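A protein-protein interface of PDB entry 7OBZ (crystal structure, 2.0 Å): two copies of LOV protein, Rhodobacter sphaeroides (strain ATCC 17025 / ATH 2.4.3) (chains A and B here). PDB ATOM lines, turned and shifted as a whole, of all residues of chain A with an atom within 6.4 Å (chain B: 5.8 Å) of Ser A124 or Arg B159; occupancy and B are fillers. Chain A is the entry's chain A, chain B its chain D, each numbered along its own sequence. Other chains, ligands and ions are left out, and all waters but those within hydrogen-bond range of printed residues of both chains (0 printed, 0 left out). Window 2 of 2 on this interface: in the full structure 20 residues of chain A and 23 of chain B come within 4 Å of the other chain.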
ATOM      1  N   PHE A 119      30.821  27.651   3.278  1.00  0.00           N
ATOM      2  CA  PHE A 119      30.298  27.443   1.938  1.00  0.00           C
ATOM      3  C   PHE A 119      31.469  27.082   1.037  1.00  0.00           C
ATOM      4  O   PHE A 119      32.459  27.823   0.973  1.00  0.00           O
ATOM      5  CB  PHE A 119      29.562  28.689   1.406  1.00  0.00           C
ATOM      6  CG  PHE A 119      29.142  28.561  -0.016  1.00  0.00           C
ATOM      7  CD1 PHE A 119      28.035  27.793  -0.348  1.00  0.00           C
ATOM      8  CD2 PHE A 119      29.859  29.184  -1.031  1.00  0.00           C
ATOM      9  CE1 PHE A 119      27.639  27.660  -1.656  1.00  0.00           C
ATOM     10  CE2 PHE A 119      29.472  29.056  -2.350  1.00  0.00           C
ATOM     11  CZ  PHE A 119      28.368  28.300  -2.669  1.00  0.00           C
ATOM     12  N   GLU A 120      31.360  25.942   0.361  1.00  0.00           N
ATOM     13  CA  GLU A 120      32.434  25.442  -0.483  1.00  0.00           C
ATOM     14  C   GLU A 120      32.307  26.091  -1.855  1.00  0.00           C
ATOM     15  O   GLU A 120      31.335  25.857  -2.583  1.00  0.00           O
ATOM     16  CB  GLU A 120      32.397  23.916  -0.579  1.00  0.00           C
ATOM     17  CG  GLU A 120      33.608  23.314  -1.311  1.00  0.00           C
ATOM     18  CD  GLU A 120      33.533  21.783  -1.503  1.00  0.00           C
ATOM     19  OE1 GLU A 120      32.926  21.096  -0.657  1.00  0.00           O
ATOM     20  OE2 GLU A 120      34.062  21.271  -2.522  1.00  0.00           O
ATOM     21  N   LEU A 121      33.280  26.928  -2.193  1.00  0.00           N
ATOM     22  CA  LEU A 121      33.409  27.440  -3.547  1.00  0.00           C
ATOM     23  C   LEU A 121      33.853  26.329  -4.497  1.00  0.00           C
ATOM     24  O   LEU A 121      34.233  25.227  -4.083  1.00  0.00           O
ATOM     25  CB  LEU A 121      34.387  28.608  -3.564  1.00  0.00           C
ATOM     26  CG  LEU A 121      34.004  29.629  -2.492  1.00  0.00           C
ATOM     27  CD1 LEU A 121      35.179  30.487  -2.064  1.00  0.00           C
ATOM     28  CD2 LEU A 121      32.866  30.492  -3.023  1.00  0.00           C
ATOM     29  N   GLY A 122      33.776  26.624  -5.793  1.00  0.00           N
ATOM     30  CA  GLY A 122      34.255  25.717  -6.823  1.00  0.00           C
ATOM     31  C   GLY A 122      33.338  24.568  -7.184  1.00  0.00           C
ATOM     32  O   GLY A 122      33.761  23.665  -7.911  1.00  0.00           O
ATOM     33  N   ARG A 123      32.092  24.589  -6.734  1.00  0.00           N
ATOM     34  CA  ARG A 123      31.220  23.432  -6.813  1.00  0.00           C
ATOM     35  C   ARG A 123      29.859  23.768  -7.412  1.00  0.00           C
ATOM     36  O   ARG A 123      29.018  22.873  -7.546  1.00  0.00           O
ATOM     37  CB  ARG A 123      31.058  22.832  -5.404  1.00  0.00           C
ATOM     38  CG  ARG A 123      30.593  21.396  -5.310  1.00  0.00           C
ATOM     39  CD  ARG A 123      29.829  21.221  -4.001  1.00  0.00           C
ATOM     40  NE  ARG A 123      29.212  22.487  -3.616  1.00  0.00           N
ATOM     41  CZ  ARG A 123      29.317  23.059  -2.423  1.00  0.00           C
ATOM     42  NH1 ARG A 123      29.910  22.439  -1.411  1.00  0.00           N
ATOM     43  NH2 ARG A 123      28.798  24.281  -2.236  1.00  0.00           N
ATOM     44  N   SER A 124      29.623  25.029  -7.784  1.00  0.00           N
ATOM     45  CA  SER A 124      28.327  25.463  -8.298  1.00  0.00           C
ATOM     46  C   SER A 124      28.415  25.978  -9.730  1.00  0.00           C
ATOM     47  O   SER A 124      27.509  26.687 -10.187  1.00  0.00           O
ATOM     48  CB  SER A 124      27.718  26.531  -7.387  1.00  0.00           C
ATOM     49  OG  SER A 124      27.863  26.172  -6.027  1.00  0.00           O
ATOM     50  N   GLY A 125      29.488  25.637 -10.442  1.00  0.00           N
ATOM     51  CA  GLY A 125      29.630  25.952 -11.851  1.00  0.00           C
ATOM     52  C   GLY A 125      29.666  27.431 -12.168  1.00  0.00           C
ATOM     53  O   GLY A 125      30.607  28.140 -11.787  1.00  0.00           O
ATOM     54  N   ASN A 126      28.646  27.909 -12.878  1.00  0.00           N
ATOM     55  CA  ASN A 126      28.552  29.312 -13.246  1.00  0.00           C
ATOM     56  C   ASN A 126      27.701  30.112 -12.277  1.00  0.00           C
ATOM     57  O   ASN A 126      27.523  31.315 -12.480  1.00  0.00           O
ATOM     58  CB  ASN A 126      27.994  29.450 -14.665  1.00  0.00           C
ATOM     59  CG  ASN A 126      28.964  28.951 -15.725  1.00  0.00           C
ATOM     60  OD1 ASN A 126      30.182  29.110 -15.598  1.00  0.00           O
ATOM     61  ND2 ASN A 126      28.425  28.349 -16.780  1.00  0.00           N
ATOM     62  N   SER A 127      27.178  29.479 -11.227  1.00  0.00           N
ATOM     63  CA  SER A 127      26.285  30.134 -10.280  1.00  0.00           C
ATOM     64  C   SER A 127      26.943  30.348  -8.923  1.00  0.00           C
ATOM     65  O   SER A 127      26.266  30.308  -7.894  1.00  0.00           O
ATOM     66  CB  SER A 127      24.992  29.335 -10.112  1.00  0.00           C
ATOM     67  OG  SER A 127      24.397  29.061 -11.364  1.00  0.00           O
ATOM     68  N   GLU A 128      28.257  30.585  -8.905  1.00  0.00           N
ATOM     69  CA  GLU A 128      28.951  30.735  -7.630  1.00  0.00           C
ATOM     70  C   GLU A 128      28.371  31.884  -6.824  1.00  0.00           C
ATOM     71  O   GLU A 128      28.178  31.766  -5.610  1.00  0.00           O
ATOM     72  CB  GLU A 128      30.447  30.944  -7.856  1.00  0.00           C
ATOM     73  CG  GLU A 128      31.182  29.703  -8.331  1.00  0.00           C
ATOM     74  CD  GLU A 128      31.178  28.586  -7.297  1.00  0.00           C
ATOM     75  OE1 GLU A 128      31.155  28.898  -6.083  1.00  0.00           O
ATOM     76  OE2 GLU A 128      31.208  27.402  -7.703  1.00  0.00           O
ATOM     77  N   ALA A 130      25.251  33.190  -6.988  1.00  0.00           N
ATOM     78  CA  ALA A 130      23.915  32.903  -6.490  1.00  0.00           C
ATOM     79  C   ALA A 130      23.937  31.807  -5.428  1.00  0.00           C
ATOM     80  O   ALA A 130      23.107  31.826  -4.512  1.00  0.00           O
ATOM     81  CB  ALA A 130      22.994  32.532  -7.656  1.00  0.00           C
ATOM     82  N   ALA A 131      24.884  30.866  -5.522  1.00  0.00           N
ATOM     83  CA  ALA A 131      24.972  29.771  -4.550  1.00  0.00           C
ATOM     84  C   ALA A 131      25.409  30.275  -3.181  1.00  0.00           C
ATOM     85  O   ALA A 131      24.822  29.903  -2.162  1.00  0.00           O
ATOM     86  CB  ALA A 131      25.942  28.696  -5.053  1.00  0.00           C
ATOM     87  N   ALA A 132      26.420  31.145  -3.143  1.00  0.00           N
ATOM     88  CA  ALA A 132      26.868  31.716  -1.879  1.00  0.00           C
ATOM     89  C   ALA A 132      25.773  32.565  -1.235  1.00  0.00           C
ATOM     90  O   ALA A 132      25.522  32.471  -0.028  1.00  0.00           O
ATOM     91  CB  ALA A 132      28.135  32.536  -2.110  1.00  0.00           C
ATOM     92  N   GLU B 154      19.155  18.753  -0.491  1.00  0.00           N
ATOM     93  CA  GLU B 154      18.899  20.130  -0.061  1.00  0.00           C
ATOM     94  C   GLU B 154      19.954  21.095  -0.582  1.00  0.00           C
ATOM     95  O   GLU B 154      19.627  22.209  -1.015  1.00  0.00           O
ATOM     96  CB  GLU B 154      18.831  20.201   1.463  1.00  0.00           C
ATOM     97  CG  GLU B 154      18.496  21.581   2.039  1.00  0.00           C
ATOM     98  CD  GLU B 154      18.343  21.530   3.555  1.00  0.00           C
ATOM     99  OE1 GLU B 154      18.353  20.403   4.100  1.00  0.00           O
ATOM    100  OE2 GLU B 154      18.236  22.594   4.202  1.00  0.00           O
ATOM    101  N   MET B 155      21.226  20.690  -0.555  1.00  0.00           N
ATOM    102  CA  MET B 155      22.286  21.591  -0.995  1.00  0.00           C
ATOM    103  C   MET B 155      22.186  21.910  -2.483  1.00  0.00           C
ATOM    104  O   MET B 155      22.269  23.078  -2.885  1.00  0.00           O
ATOM    105  CB  MET B 155      23.647  20.993  -0.697  1.00  0.00           C
ATOM    106  CG  MET B 155      24.754  21.942  -1.063  1.00  0.00           C
ATOM    107  SD  MET B 155      26.305  21.095  -0.833  1.00  0.00           S
ATOM    108  CE  MET B 155      26.668  20.855  -2.569  1.00  0.00           C
ATOM    109  N   ASP B 156      22.072  20.886  -3.325  1.00  0.00           N
ATOM    110  CA  ASP B 156      22.012  21.134  -4.762  1.00  0.00           C
ATOM    111  C   ASP B 156      20.689  21.771  -5.160  1.00  0.00           C
ATOM    112  O   ASP B 156      20.646  22.595  -6.082  1.00  0.00           O
ATOM    113  CB  ASP B 156      22.226  19.838  -5.537  1.00  0.00           C
ATOM    114  CG  ASP B 156      22.376  20.077  -7.021  1.00  0.00           C
ATOM    115  OD1 ASP B 156      23.250  20.885  -7.406  1.00  0.00           O
ATOM    116  OD2 ASP B 156      21.617  19.461  -7.798  1.00  0.00           O
ATOM    117  N   SER B 157      19.607  21.405  -4.475  1.00  0.00           N
ATOM    118  CA  SER B 157      18.323  22.051  -4.704  1.00  0.00           C
ATOM    119  C   SER B 157      18.410  23.541  -4.393  1.00  0.00           C
ATOM    120  O   SER B 157      17.930  24.386  -5.164  1.00  0.00           O
ATOM    121  CB  SER B 157      17.256  21.363  -3.852  1.00  0.00           C
ATOM    122  OG  SER B 157      16.128  22.180  -3.642  1.00  0.00           O
ATOM    123  N   ARG B 158      19.029  23.881  -3.261  1.00  0.00           N
ATOM    124  CA  ARG B 158      19.220  25.284  -2.903  1.00  0.00           C
ATOM    125  C   ARG B 158      20.042  26.003  -3.963  1.00  0.00           C
ATOM    126  O   ARG B 158      19.766  27.159  -4.304  1.00  0.00           O
ATOM    127  CB  ARG B 158      19.897  25.381  -1.531  1.00  0.00           C
ATOM    128  CG  ARG B 158      20.475  26.739  -1.200  1.00  0.00           C
ATOM    129  CD  ARG B 158      20.915  26.809   0.250  1.00  0.00           C
ATOM    130  NE  ARG B 158      22.047  25.939   0.536  1.00  0.00           N
ATOM    131  CZ  ARG B 158      21.998  24.924   1.385  1.00  0.00           C
ATOM    132  NH1 ARG B 158      20.899  24.649   2.068  1.00  0.00           N
ATOM    133  NH2 ARG B 158      23.073  24.161   1.546  1.00  0.00           N
ATOM    134  N   ARG B 159      21.055  25.328  -4.503  1.00  0.00           N
ATOM    135  CA  ARG B 159      21.899  25.959  -5.503  1.00  0.00           C
ATOM    136  C   ARG B 159      21.101  26.256  -6.769  1.00  0.00           C
ATOM    137  O   ARG B 159      21.180  27.359  -7.319  1.00  0.00           O
ATOM    138  CB  ARG B 159      23.109  25.068  -5.802  1.00  0.00           C
ATOM    139  CG  ARG B 159      23.893  25.559  -6.978  1.00  0.00           C
ATOM    140  CD  ARG B 159      24.327  24.437  -7.888  1.00  0.00           C
ATOM    141  NE  ARG B 159      24.579  24.941  -9.233  1.00  0.00           N
ATOM    142  CZ  ARG B 159      25.177  24.248 -10.193  1.00  0.00           C
ATOM    143  NH1 ARG B 159      25.628  23.018  -9.980  1.00  0.00           N
ATOM    144  NH2 ARG B 159      25.351  24.810 -11.387  1.00  0.00           N
ATOM    145  N   HIS B 160      20.302  25.287  -7.229  1.00  0.00           N
ATOM    146  CA  HIS B 160      19.506  25.466  -8.441  1.00  0.00           C
ATOM    147  C   HIS B 160      18.330  26.415  -8.237  1.00  0.00           C
ATOM    148  O   HIS B 160      17.847  27.007  -9.210  1.00  0.00           O
ATOM    149  CB  HIS B 160      18.978  24.120  -8.941  1.00  0.00           C
ATOM    150  CG  HIS B 160      20.051  23.190  -9.422  1.00  0.00           C
ATOM    151  ND1 HIS B 160      21.037  23.582 -10.304  1.00  0.00           N
ATOM    152  CD2 HIS B 160      20.294  21.887  -9.143  1.00  0.00           C
ATOM    153  CE1 HIS B 160      21.842  22.562 -10.544  1.00  0.00           C
ATOM    154  NE2 HIS B 160      21.413  21.522  -9.852  1.00  0.00           N
ATOM    155  N   LEU B 161      17.846  26.563  -7.009  1.00  0.00           N
ATOM    156  CA  LEU B 161      16.745  27.485  -6.794  1.00  0.00           C
ATOM    157  C   LEU B 161      17.245  28.908  -6.624  1.00  0.00           C
ATOM    158  O   LEU B 161      16.566  29.851  -7.042  1.00  0.00           O
ATOM    159  CB  LEU B 161      15.920  27.072  -5.580  1.00  0.00           C
ATOM    160  CG  LEU B 161      14.560  27.768  -5.521  1.00  0.00           C
ATOM    161  CD1 LEU B 161      13.675  27.288  -6.658  1.00  0.00           C
ATOM    162  CD2 LEU B 161      13.873  27.587  -4.172  1.00  0.00           C
ATOM    163  N   ALA B 162      18.413  29.089  -6.007  1.00  0.00           N
ATOM    164  CA  ALA B 162      19.007  30.418  -5.978  1.00  0.00           C
ATOM    165  C   ALA B 162      19.408  30.867  -7.381  1.00  0.00           C
ATOM    166  O   ALA B 162      19.261  32.039  -7.734  1.00  0.00           O
ATOM    167  CB  ALA B 162      20.208  30.444  -5.039  1.00  0.00           C
ATOM    168  N   GLN B 163      19.915  29.946  -8.195  1.00  0.00           N
ATOM    169  CA  GLN B 163      20.315  30.300  -9.550  1.00  0.00           C
ATOM    170  C   GLN B 163      19.107  30.713 -10.381  1.00  0.00           C
ATOM    171  O   GLN B 163      19.155  31.706 -11.123  1.00  0.00           O
ATOM    172  CB  GLN B 163      21.067  29.116 -10.170  1.00  0.00           C
ATOM    173  CG  GLN B 163      21.058  28.988 -11.685  1.00  0.00           C
ATOM    174  CD  GLN B 163      21.678  27.664 -12.140  1.00  0.00           C
ATOM    175  OE1 GLN B 163      21.089  26.594 -11.964  1.00  0.00           O
ATOM    176  NE2 GLN B 163      22.868  27.734 -12.726  1.00  0.00           N
ATOM    177  N   ALA B 164      18.006  29.976 -10.255  1.00  0.00           N
ATOM    178  CA  ALA B 164      16.798  30.347 -10.973  1.00  0.00           C
ATOM    179  C   ALA B 164      16.333  31.735 -10.567  1.00  0.00           C
ATOM    180  O   ALA B 164      15.931  32.539 -11.415  1.00  0.00           O
ATOM    181  CB  ALA B 164      15.697  29.329 -10.714  1.00  0.00           C
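The backbone carbonyl oxygen (O) of Ser A124 lies within hydrogen-bond range of the guanidinium group (NH2) of Arg B159. NE2 of Gln B163 is in hydrogen-bond range of OG of Ser A127, at 2.4 Å.
The guanidinium group (NH1) of Arg A123 is in salt-bridge range of the side-chain carboxylate (OE1) of Glu A120. The backbone NH (N) of Arg A123 lies within hydrogen-bond range of the side-chain carboxylate (OE2) of Glu A128 (3.1 Å). N of Ser A124 lies within hydrogen-bond range of OE2 of Glu A128 (2.9 Å). The side-chain amide oxygen (OE1) of Gln B163 is in hydrogen-bond range of a ring nitrogen (ND1) of His B160.
Among the printed residues, merely in contact across the chains: Arg A123 with Met B155 (3.2 Å), Ala A130 with Ala B162 (3.3 Å) and Ala A130 with Gln B163 (3.97 Å).
Ser A124 touches just one residue of chain B: Arg B159. Gly A125 touches none of the printed residues of chain B. Of the printed residues of chain B, Ser A127 touches Gln B163 (2.4 Å). Of the printed residues of chain B, Ala A130 touches Ala B162 and Gln B163. Of the printed residues of chain A, Met B155 touches Arg A123. Of chain A, only Ser A124 (3.1 Å) comes within 4 Å of Arg B159. The nearest printed residue of chain B that does not touch Ala A130 is Arg B159 (5.5 Å).
Of the 11 printed residues of chain B, 4 touch a printed residue of chain A. Of the 13 printed residues of chain A, 4 touch a printed residue of chain B. Among the printed residues, 5 pairs touch across the chains.
No position is printed for both chains.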
